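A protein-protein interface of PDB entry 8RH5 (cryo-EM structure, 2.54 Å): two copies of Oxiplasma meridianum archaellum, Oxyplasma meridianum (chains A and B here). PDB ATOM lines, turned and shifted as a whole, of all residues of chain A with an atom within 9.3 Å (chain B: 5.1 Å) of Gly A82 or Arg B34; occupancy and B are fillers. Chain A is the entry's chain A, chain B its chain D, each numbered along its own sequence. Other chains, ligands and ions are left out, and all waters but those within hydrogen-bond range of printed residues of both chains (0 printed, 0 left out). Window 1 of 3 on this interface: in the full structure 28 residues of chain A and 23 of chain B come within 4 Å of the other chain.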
ATOM      1  N   GLY A  39      -9.493  42.783  -1.568  1.00  0.00           N
ATOM      2  CA  GLY A  39      -8.746  41.566  -1.289  1.00  0.00           C
ATOM      3  C   GLY A  39      -9.604  40.308  -1.407  1.00  0.00           C
ATOM      4  O   GLY A  39      -9.151  39.302  -1.950  1.00  0.00           O
ATOM      5  N   SER A  40     -10.842  40.391  -0.899  1.00  0.00           N
ATOM      6  CA  SER A  40     -11.772  39.273  -0.857  1.00  0.00           C
ATOM      7  C   SER A  40     -12.333  38.968  -2.245  1.00  0.00           C
ATOM      8  O   SER A  40     -12.562  37.805  -2.574  1.00  0.00           O
ATOM      9  CB  SER A  40     -12.873  39.517   0.145  1.00  0.00           C
ATOM     10  OG  SER A  40     -13.606  40.689  -0.180  1.00  0.00           O
ATOM     11  N   GLN A  41     -12.549  40.023  -3.044  1.00  0.00           N
ATOM     12  CA  GLN A  41     -13.128  39.920  -4.376  1.00  0.00           C
ATOM     13  C   GLN A  41     -12.124  39.309  -5.354  1.00  0.00           C
ATOM     14  O   GLN A  41     -12.518  38.566  -6.253  1.00  0.00           O
ATOM     15  CB  GLN A  41     -13.618  41.285  -4.865  1.00  0.00           C
ATOM     16  CG  GLN A  41     -15.018  41.642  -4.380  1.00  0.00           C
ATOM     17  CD  GLN A  41     -15.396  43.081  -4.634  1.00  0.00           C
ATOM     18  OE1 GLN A  41     -15.117  43.647  -5.689  1.00  0.00           O
ATOM     19  NE2 GLN A  41     -16.054  43.688  -3.660  1.00  0.00           N
ATOM     20  N   THR A  42     -10.837  39.632  -5.164  1.00  0.00           N
ATOM     21  CA  THR A  42      -9.757  39.172  -6.027  1.00  0.00           C
ATOM     22  C   THR A  42      -9.484  37.689  -5.781  1.00  0.00           C
ATOM     23  O   THR A  42      -9.180  36.955  -6.721  1.00  0.00           O
ATOM     24  CB  THR A  42      -8.508  40.052  -5.872  1.00  0.00           C
ATOM     25  OG1 THR A  42      -8.896  41.419  -6.024  1.00  0.00           O
ATOM     26  CG2 THR A  42      -7.415  39.736  -6.868  1.00  0.00           C
ATOM     27  N   THR A  43      -9.603  37.264  -4.514  1.00  0.00           N
ATOM     28  CA  THR A  43      -9.386  35.886  -4.095  1.00  0.00           C
ATOM     29  C   THR A  43     -10.426  34.973  -4.745  1.00  0.00           C
ATOM     30  O   THR A  43     -10.102  33.858  -5.155  1.00  0.00           O
ATOM     31  CB  THR A  43      -9.345  35.771  -2.563  1.00  0.00           C
ATOM     32  OG1 THR A  43      -8.438  36.751  -2.057  1.00  0.00           O
ATOM     33  CG2 THR A  43      -8.919  34.404  -2.071  1.00  0.00           C
ATOM     34  N   ASN A  44     -11.668  35.469  -4.843  1.00  0.00           N
ATOM     35  CA  ASN A  44     -12.768  34.757  -5.475  1.00  0.00           C
ATOM     36  C   ASN A  44     -12.598  34.749  -6.993  1.00  0.00           C
ATOM     37  O   ASN A  44     -13.017  33.800  -7.650  1.00  0.00           O
ATOM     38  CB  ASN A  44     -14.129  35.331  -5.068  1.00  0.00           C
ATOM     39  CG  ASN A  44     -14.517  35.013  -3.638  1.00  0.00           C
ATOM     40  OD1 ASN A  44     -14.553  33.849  -3.240  1.00  0.00           O
ATOM     41  ND2 ASN A  44     -14.824  36.039  -2.863  1.00  0.00           N
ATOM     42  N   GLN A  45     -11.975  35.808  -7.530  1.00  0.00           N
ATOM     43  CA  GLN A  45     -11.833  36.023  -8.963  1.00  0.00           C
ATOM     44  C   GLN A  45     -10.850  35.016  -9.563  1.00  0.00           C
ATOM     45  O   GLN A  45     -11.087  34.505 -10.659  1.00  0.00           O
ATOM     46  CB  GLN A  45     -11.415  37.469  -9.241  1.00  0.00           C
ATOM     47  CG  GLN A  45     -11.608  37.910 -10.687  1.00  0.00           C
ATOM     48  CD  GLN A  45     -10.391  37.691 -11.555  1.00  0.00           C
ATOM     49  OE1 GLN A  45      -9.269  38.043 -11.194  1.00  0.00           O
ATOM     50  NE2 GLN A  45     -10.610  37.114 -12.725  1.00  0.00           N
ATOM     51  N   VAL A  46      -9.758  34.742  -8.837  1.00  0.00           N
ATOM     52  CA  VAL A  46      -8.667  33.906  -9.316  1.00  0.00           C
ATOM     53  C   VAL A  46      -9.069  32.432  -9.230  1.00  0.00           C
ATOM     54  O   VAL A  46      -8.824  31.670 -10.165  1.00  0.00           O
ATOM     55  CB  VAL A  46      -7.346  34.208  -8.573  1.00  0.00           C
ATOM     56  CG1 VAL A  46      -6.229  33.236  -8.931  1.00  0.00           C
ATOM     57  CG2 VAL A  46      -6.881  35.640  -8.793  1.00  0.00           C
ATOM     58  N   SER A  47      -9.707  32.054  -8.114  1.00  0.00           N
ATOM     59  CA  SER A  47      -9.981  30.665  -7.770  1.00  0.00           C
ATOM     60  C   SER A  47     -11.110  30.076  -8.616  1.00  0.00           C
ATOM     61  O   SER A  47     -11.075  28.890  -8.942  1.00  0.00           O
ATOM     62  CB  SER A  47     -10.257  30.518  -6.294  1.00  0.00           C
ATOM     63  OG  SER A  47     -11.374  31.304  -5.905  1.00  0.00           O
ATOM     64  N   THR A  48     -12.100  30.911  -8.962  1.00  0.00           N
ATOM     65  CA  THR A  48     -13.307  30.477  -9.653  1.00  0.00           C
ATOM     66  C   THR A  48     -13.017  30.280 -11.141  1.00  0.00           C
ATOM     67  O   THR A  48     -12.256  31.043 -11.736  1.00  0.00           O
ATOM     68  CB  THR A  48     -14.472  31.442  -9.384  1.00  0.00           C
ATOM     69  OG1 THR A  48     -14.553  31.668  -7.977  1.00  0.00           O
ATOM     70  CG2 THR A  48     -15.810  30.933  -9.874  1.00  0.00           C
ATOM     71  N   GLY A  49     -13.639  29.244 -11.723  1.00  0.00           N
ATOM     72  CA  GLY A  49     -13.527  28.930 -13.139  1.00  0.00           C
ATOM     73  C   GLY A  49     -14.434  27.774 -13.554  1.00  0.00           C
ATOM     74  O   GLY A  49     -14.870  26.987 -12.713  1.00  0.00           O
ATOM     75  N   LEU A  79     -17.569  22.776 -12.532  1.00  0.00           N
ATOM     76  CA  LEU A  79     -16.755  23.793 -11.884  1.00  0.00           C
ATOM     77  C   LEU A  79     -15.330  23.276 -11.693  1.00  0.00           C
ATOM     78  O   LEU A  79     -15.093  22.069 -11.719  1.00  0.00           O
ATOM     79  CB  LEU A  79     -17.379  24.164 -10.532  1.00  0.00           C
ATOM     80  CG  LEU A  79     -18.400  25.302 -10.543  1.00  0.00           C
ATOM     81  CD1 LEU A  79     -19.119  25.384  -9.206  1.00  0.00           C
ATOM     82  CD2 LEU A  79     -17.744  26.639 -10.864  1.00  0.00           C
ATOM     83  N   ASN A  80     -14.399  24.217 -11.497  1.00  0.00           N
ATOM     84  CA  ASN A  80     -13.012  23.922 -11.171  1.00  0.00           C
ATOM     85  C   ASN A  80     -12.907  23.608  -9.678  1.00  0.00           C
ATOM     86  O   ASN A  80     -13.835  23.880  -8.916  1.00  0.00           O
ATOM     87  CB  ASN A  80     -12.085  25.065 -11.602  1.00  0.00           C
ATOM     88  CG  ASN A  80     -10.656  24.639 -11.874  1.00  0.00           C
ATOM     89  OD1 ASN A  80     -10.267  23.504 -11.602  1.00  0.00           O
ATOM     90  ND2 ASN A  80      -9.861  25.550 -12.411  1.00  0.00           N
ATOM     91  N   THR A  81     -11.767  23.029  -9.274  1.00  0.00           N
ATOM     92  CA  THR A  81     -11.528  22.614  -7.899  1.00  0.00           C
ATOM     93  C   THR A  81     -11.264  23.834  -7.019  1.00  0.00           C
ATOM     94  O   THR A  81     -10.398  24.653  -7.328  1.00  0.00           O
ATOM     95  CB  THR A  81     -10.404  21.572  -7.803  1.00  0.00           C
ATOM     96  OG1 THR A  81      -9.251  22.070  -8.486  1.00  0.00           O
ATOM     97  CG2 THR A  81     -10.796  20.222  -8.364  1.00  0.00           C
ATOM     98  N   GLY A  82     -12.033  23.931  -5.927  1.00  0.00           N
ATOM     99  CA  GLY A  82     -11.944  25.021  -4.968  1.00  0.00           C
ATOM    100  C   GLY A  82     -12.464  26.337  -5.542  1.00  0.00           C
ATOM    101  O   GLY A  82     -11.798  27.365  -5.436  1.00  0.00           O
ATOM    102  N   SER A  83     -13.662  26.281  -6.141  1.00  0.00           N
ATOM    103  CA  SER A  83     -14.268  27.420  -6.812  1.00  0.00           C
ATOM    104  C   SER A  83     -15.531  27.867  -6.080  1.00  0.00           C
ATOM    105  O   SER A  83     -16.236  27.051  -5.487  1.00  0.00           O
ATOM    106  CB  SER A  83     -14.559  27.103  -8.258  1.00  0.00           C
ATOM    107  OG  SER A  83     -13.359  26.823  -8.966  1.00  0.00           O
ATOM    108  N   SER A  84     -15.793  29.179  -6.143  1.00  0.00           N
ATOM    109  CA  SER A  84     -17.006  29.791  -5.627  1.00  0.00           C
ATOM    110  C   SER A  84     -18.177  29.482  -6.561  1.00  0.00           C
ATOM    111  O   SER A  84     -17.960  29.274  -7.755  1.00  0.00           O
ATOM    112  CB  SER A  84     -16.814  31.279  -5.455  1.00  0.00           C
ATOM    113  OG  SER A  84     -15.796  31.549  -4.501  1.00  0.00           O
ATOM    114  N   PRO A  85     -19.439  29.424  -6.059  1.00  0.00           N
ATOM    115  CA  PRO A  85     -20.607  29.150  -6.905  1.00  0.00           C
ATOM    116  C   PRO A  85     -20.798  30.136  -8.057  1.00  0.00           C
ATOM    117  O   PRO A  85     -20.496  31.321  -7.922  1.00  0.00           O
ATOM    118  CB  PRO A  85     -21.797  29.257  -5.937  1.00  0.00           C
ATOM    119  CG  PRO A  85     -21.198  28.968  -4.579  1.00  0.00           C
ATOM    120  CD  PRO A  85     -19.812  29.574  -4.641  1.00  0.00           C
ATOM    121  N   THR A 176     -22.830  24.507  -8.035  1.00  0.00           N
ATOM    122  CA  THR A 176     -22.049  24.363  -6.814  1.00  0.00           C
ATOM    123  C   THR A 176     -21.031  23.233  -6.972  1.00  0.00           C
ATOM    124  O   THR A 176     -20.864  22.692  -8.066  1.00  0.00           O
ATOM    125  CB  THR A 176     -22.955  24.202  -5.584  1.00  0.00           C
ATOM    126  OG1 THR A 176     -23.895  23.154  -5.831  1.00  0.00           O
ATOM    127  CG2 THR A 176     -23.686  25.471  -5.202  1.00  0.00           C
ATOM    128  N   THR A 177     -20.350  22.896  -5.867  1.00  0.00           N
ATOM    129  CA  THR A 177     -19.306  21.883  -5.839  1.00  0.00           C
ATOM    130  C   THR A 177     -19.933  20.494  -5.948  1.00  0.00           C
ATOM    131  O   THR A 177     -20.774  20.122  -5.132  1.00  0.00           O
ATOM    132  CB  THR A 177     -18.411  22.042  -4.599  1.00  0.00           C
ATOM    133  OG1 THR A 177     -17.991  23.403  -4.504  1.00  0.00           O
ATOM    134  CG2 THR A 177     -17.194  21.141  -4.616  1.00  0.00           C
ATOM    135  N   GLY A 178     -19.511  19.749  -6.980  1.00  0.00           N
ATOM    136  CA  GLY A 178     -19.926  18.371  -7.193  1.00  0.00           C
ATOM    137  C   GLY A 178     -21.074  18.235  -8.192  1.00  0.00           C
ATOM    138  O   GLY A 178     -21.528  17.121  -8.454  1.00  0.00           O
ATOM    139  N   SER B  30      -7.326  35.580   5.889  1.00  0.00           N
ATOM    140  CA  SER B  30      -8.383  35.146   4.988  1.00  0.00           C
ATOM    141  C   SER B  30      -7.797  34.399   3.790  1.00  0.00           C
ATOM    142  O   SER B  30      -8.377  33.415   3.334  1.00  0.00           O
ATOM    143  CB  SER B  30      -9.232  36.313   4.548  1.00  0.00           C
ATOM    144  OG  SER B  30      -9.859  36.931   5.661  1.00  0.00           O
ATOM    145  N   LEU B  31      -6.644  34.877   3.300  1.00  0.00           N
ATOM    146  CA  LEU B  31      -5.972  34.319   2.135  1.00  0.00           C
ATOM    147  C   LEU B  31      -5.205  33.050   2.508  1.00  0.00           C
ATOM    148  O   LEU B  31      -4.874  32.255   1.627  1.00  0.00           O
ATOM    149  CB  LEU B  31      -5.034  35.375   1.539  1.00  0.00           C
ATOM    150  CG  LEU B  31      -5.647  36.289   0.477  1.00  0.00           C
ATOM    151  CD1 LEU B  31      -4.959  37.646   0.471  1.00  0.00           C
ATOM    152  CD2 LEU B  31      -5.577  35.651  -0.903  1.00  0.00           C
ATOM    153  N   GLN B  32      -4.928  32.879   3.807  1.00  0.00           N
ATOM    154  CA  GLN B  32      -4.173  31.752   4.338  1.00  0.00           C
ATOM    155  C   GLN B  32      -4.960  30.454   4.151  1.00  0.00           C
ATOM    156  O   GLN B  32      -4.400  29.455   3.702  1.00  0.00           O
ATOM    157  CB  GLN B  32      -3.822  32.000   5.809  1.00  0.00           C
ATOM    158  CG  GLN B  32      -3.014  30.880   6.459  1.00  0.00           C
ATOM    159  CD  GLN B  32      -2.618  31.168   7.887  1.00  0.00           C
ATOM    160  OE1 GLN B  32      -1.441  31.144   8.241  1.00  0.00           O
ATOM    161  NE2 GLN B  32      -3.604  31.437   8.731  1.00  0.00           N
ATOM    162  N   GLN B  33      -6.255  30.495   4.490  1.00  0.00           N
ATOM    163  CA  GLN B  33      -7.112  29.319   4.533  1.00  0.00           C
ATOM    164  C   GLN B  33      -7.471  28.860   3.120  1.00  0.00           C
ATOM    165  O   GLN B  33      -7.631  27.662   2.887  1.00  0.00           O
ATOM    166  CB  GLN B  33      -8.365  29.588   5.371  1.00  0.00           C
ATOM    167  CG  GLN B  33      -8.087  29.862   6.846  1.00  0.00           C
ATOM    168  CD  GLN B  33      -7.431  28.714   7.577  1.00  0.00           C
ATOM    169  OE1 GLN B  33      -7.854  27.563   7.486  1.00  0.00           O
ATOM    170  NE2 GLN B  33      -6.384  29.026   8.324  1.00  0.00           N
ATOM    171  N   ARG B  34      -7.592  29.823   2.196  1.00  0.00           N
ATOM    172  CA  ARG B  34      -7.943  29.561   0.807  1.00  0.00           C
ATOM    173  C   ARG B  34      -6.781  28.867   0.096  1.00  0.00           C
ATOM    174  O   ARG B  34      -6.999  27.901  -0.632  1.00  0.00           O
ATOM    175  CB  ARG B  34      -8.390  30.854   0.112  1.00  0.00           C
ATOM    176  CG  ARG B  34      -8.703  30.715  -1.374  1.00  0.00           C
ATOM    177  CD  ARG B  34     -10.031  30.062  -1.718  1.00  0.00           C
ATOM    178  NE  ARG B  34     -11.160  30.979  -1.607  1.00  0.00           N
ATOM    179  CZ  ARG B  34     -12.355  30.801  -2.168  1.00  0.00           C
ATOM    180  NH1 ARG B  34     -13.301  31.709  -1.994  1.00  0.00           N
ATOM    181  NH2 ARG B  34     -12.604  29.731  -2.902  1.00  0.00           N
ATOM    182  N   ALA B  35      -5.557  29.361   0.331  1.00  0.00           N
ATOM    183  CA  ALA B  35      -4.352  28.876  -0.327  1.00  0.00           C
ATOM    184  C   ALA B  35      -3.983  27.475   0.160  1.00  0.00           C
ATOM    185  O   ALA B  35      -3.442  26.681  -0.610  1.00  0.00           O
ATOM    186  CB  ALA B  35      -3.219  29.851  -0.120  1.00  0.00           C
ATOM    187  N   THR B  36      -4.284  27.189   1.434  1.00  0.00           N
ATOM    188  CA  THR B  36      -3.993  25.907   2.061  1.00  0.00           C
ATOM    189  C   THR B  36      -4.943  24.836   1.524  1.00  0.00           C
ATOM    190  O   THR B  36      -4.514  23.720   1.230  1.00  0.00           O
ATOM    191  CB  THR B  36      -4.010  26.022   3.593  1.00  0.00           C
ATOM    192  OG1 THR B  36      -3.158  27.104   3.976  1.00  0.00           O
ATOM    193  CG2 THR B  36      -3.554  24.763   4.298  1.00  0.00           C
ATOM    194  N   SER B  37      -6.229  25.198   1.393  1.00  0.00           N
ATOM    195  CA  SER B  37      -7.284  24.287   0.975  1.00  0.00           C
ATOM    196  C   SER B  37      -7.157  23.936  -0.508  1.00  0.00           C
ATOM    197  O   SER B  37      -7.456  22.809  -0.897  1.00  0.00           O
ATOM    198  CB  SER B  37      -8.648  24.843   1.298  1.00  0.00           C
ATOM    199  OG  SER B  37      -8.853  26.094   0.658  1.00  0.00           O
ATOM    200  N   THR B  38      -6.713  24.912  -1.315  1.00  0.00           N
ATOM    201  CA  THR B  38      -6.568  24.766  -2.758  1.00  0.00           C
ATOM    202  C   THR B  38      -5.465  23.755  -3.075  1.00  0.00           C
ATOM    203  O   THR B  38      -5.619  22.941  -3.984  1.00  0.00           O
ATOM    204  CB  THR B  38      -6.364  26.129  -3.437  1.00  0.00           C
ATOM    205  OG1 THR B  38      -7.444  26.984  -3.059  1.00  0.00           O
ATOM    206  CG2 THR B  38      -6.305  26.053  -4.948  1.00  0.00           C
ATOM    207  N   GLN B  41      -6.626  20.076  -2.105  1.00  0.00           N
ATOM    208  CA  GLN B  41      -7.701  19.603  -2.965  1.00  0.00           C
ATOM    209  C   GLN B  41      -7.157  19.184  -4.330  1.00  0.00           C
ATOM    210  O   GLN B  41      -7.660  18.231  -4.924  1.00  0.00           O
ATOM    211  CB  GLN B  41      -8.793  20.668  -3.105  1.00  0.00           C
ATOM    212  CG  GLN B  41      -9.811  20.656  -1.972  1.00  0.00           C
ATOM    213  CD  GLN B  41     -10.723  21.858  -1.966  1.00  0.00           C
ATOM    214  OE1 GLN B  41     -11.197  22.317  -3.004  1.00  0.00           O
ATOM    215  NE2 GLN B  41     -10.990  22.377  -0.779  1.00  0.00           N
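Of the printed residues of chain B, Thr A43 touches Leu B31 (3.3 Å) and Arg B34 (3.8 Å).
Printed residues of chain B within 4 Å of Ser A47: Arg B34 (3.6 Å).
Of chain B, only Arg B34 (3.6 Å) and Gln B41 (3.4 Å) come within 4 Å of Gly A82.
Of the printed residues of chain A, Leu B31 touches Thr A43 (3.3 Å).
Arg B34 touches just these residues of chain A: Thr A43 (3.8 Å), Asn A44 (2.8 Å), Ser A47 (3.6 Å), Gly A82 (3.6 Å) and Ser A84 (3.5 Å).
No residue of chain A comes within 4 Å of Ala B35.
No residue of chain A comes within 4 Å of Ser B37.
Printed residues of chain A within 4 Å of Gln B41: Gly A82.
The nearest printed residue of chain B that does not touch Thr A43 is Ser B30 (5.5 Å).
The side-chain amide oxygen (OD1) of Asn A44 is in hydrogen-bond range of the guanidinium group (NH1) of Arg B34 (2.8 Å).
N of Gly A82 sits close to OE1 of Gln B41 (3.4 Å).
Among the printed residues, pairs that only touch across the chains: Thr A43 with Leu B31 (3.3 Å), Ser A84 with Arg B34 (3.5 Å), Gly A82 with Arg B34 (3.6 Å), Ser A47 with Arg B34 (3.6 Å) and Thr A43 with Arg B34 (3.8 Å).
OG1 of Thr A43 is in hydrogen-bond range of O of Gly A39 (2.7 Å).
O of Ser A40 sits at hydrogen-bond distance from ND2 of Asn A44 (2.9 Å).
O of Asn A44 sits at hydrogen-bond distance from OG of Ser A47 (3.5 Å).
OG1 of Thr A48 lies within hydrogen-bond range of O of Asn A44.
OG of Ser A83 sits at hydrogen-bond distance from O of Ser A47 (3.1 Å).
The backbone carbonyl oxygen of Arg B34 is in hydrogen-bond range of the side-chain hydroxyl of Thr B38 (2.6 Å).
Position printed for both chains: 41.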
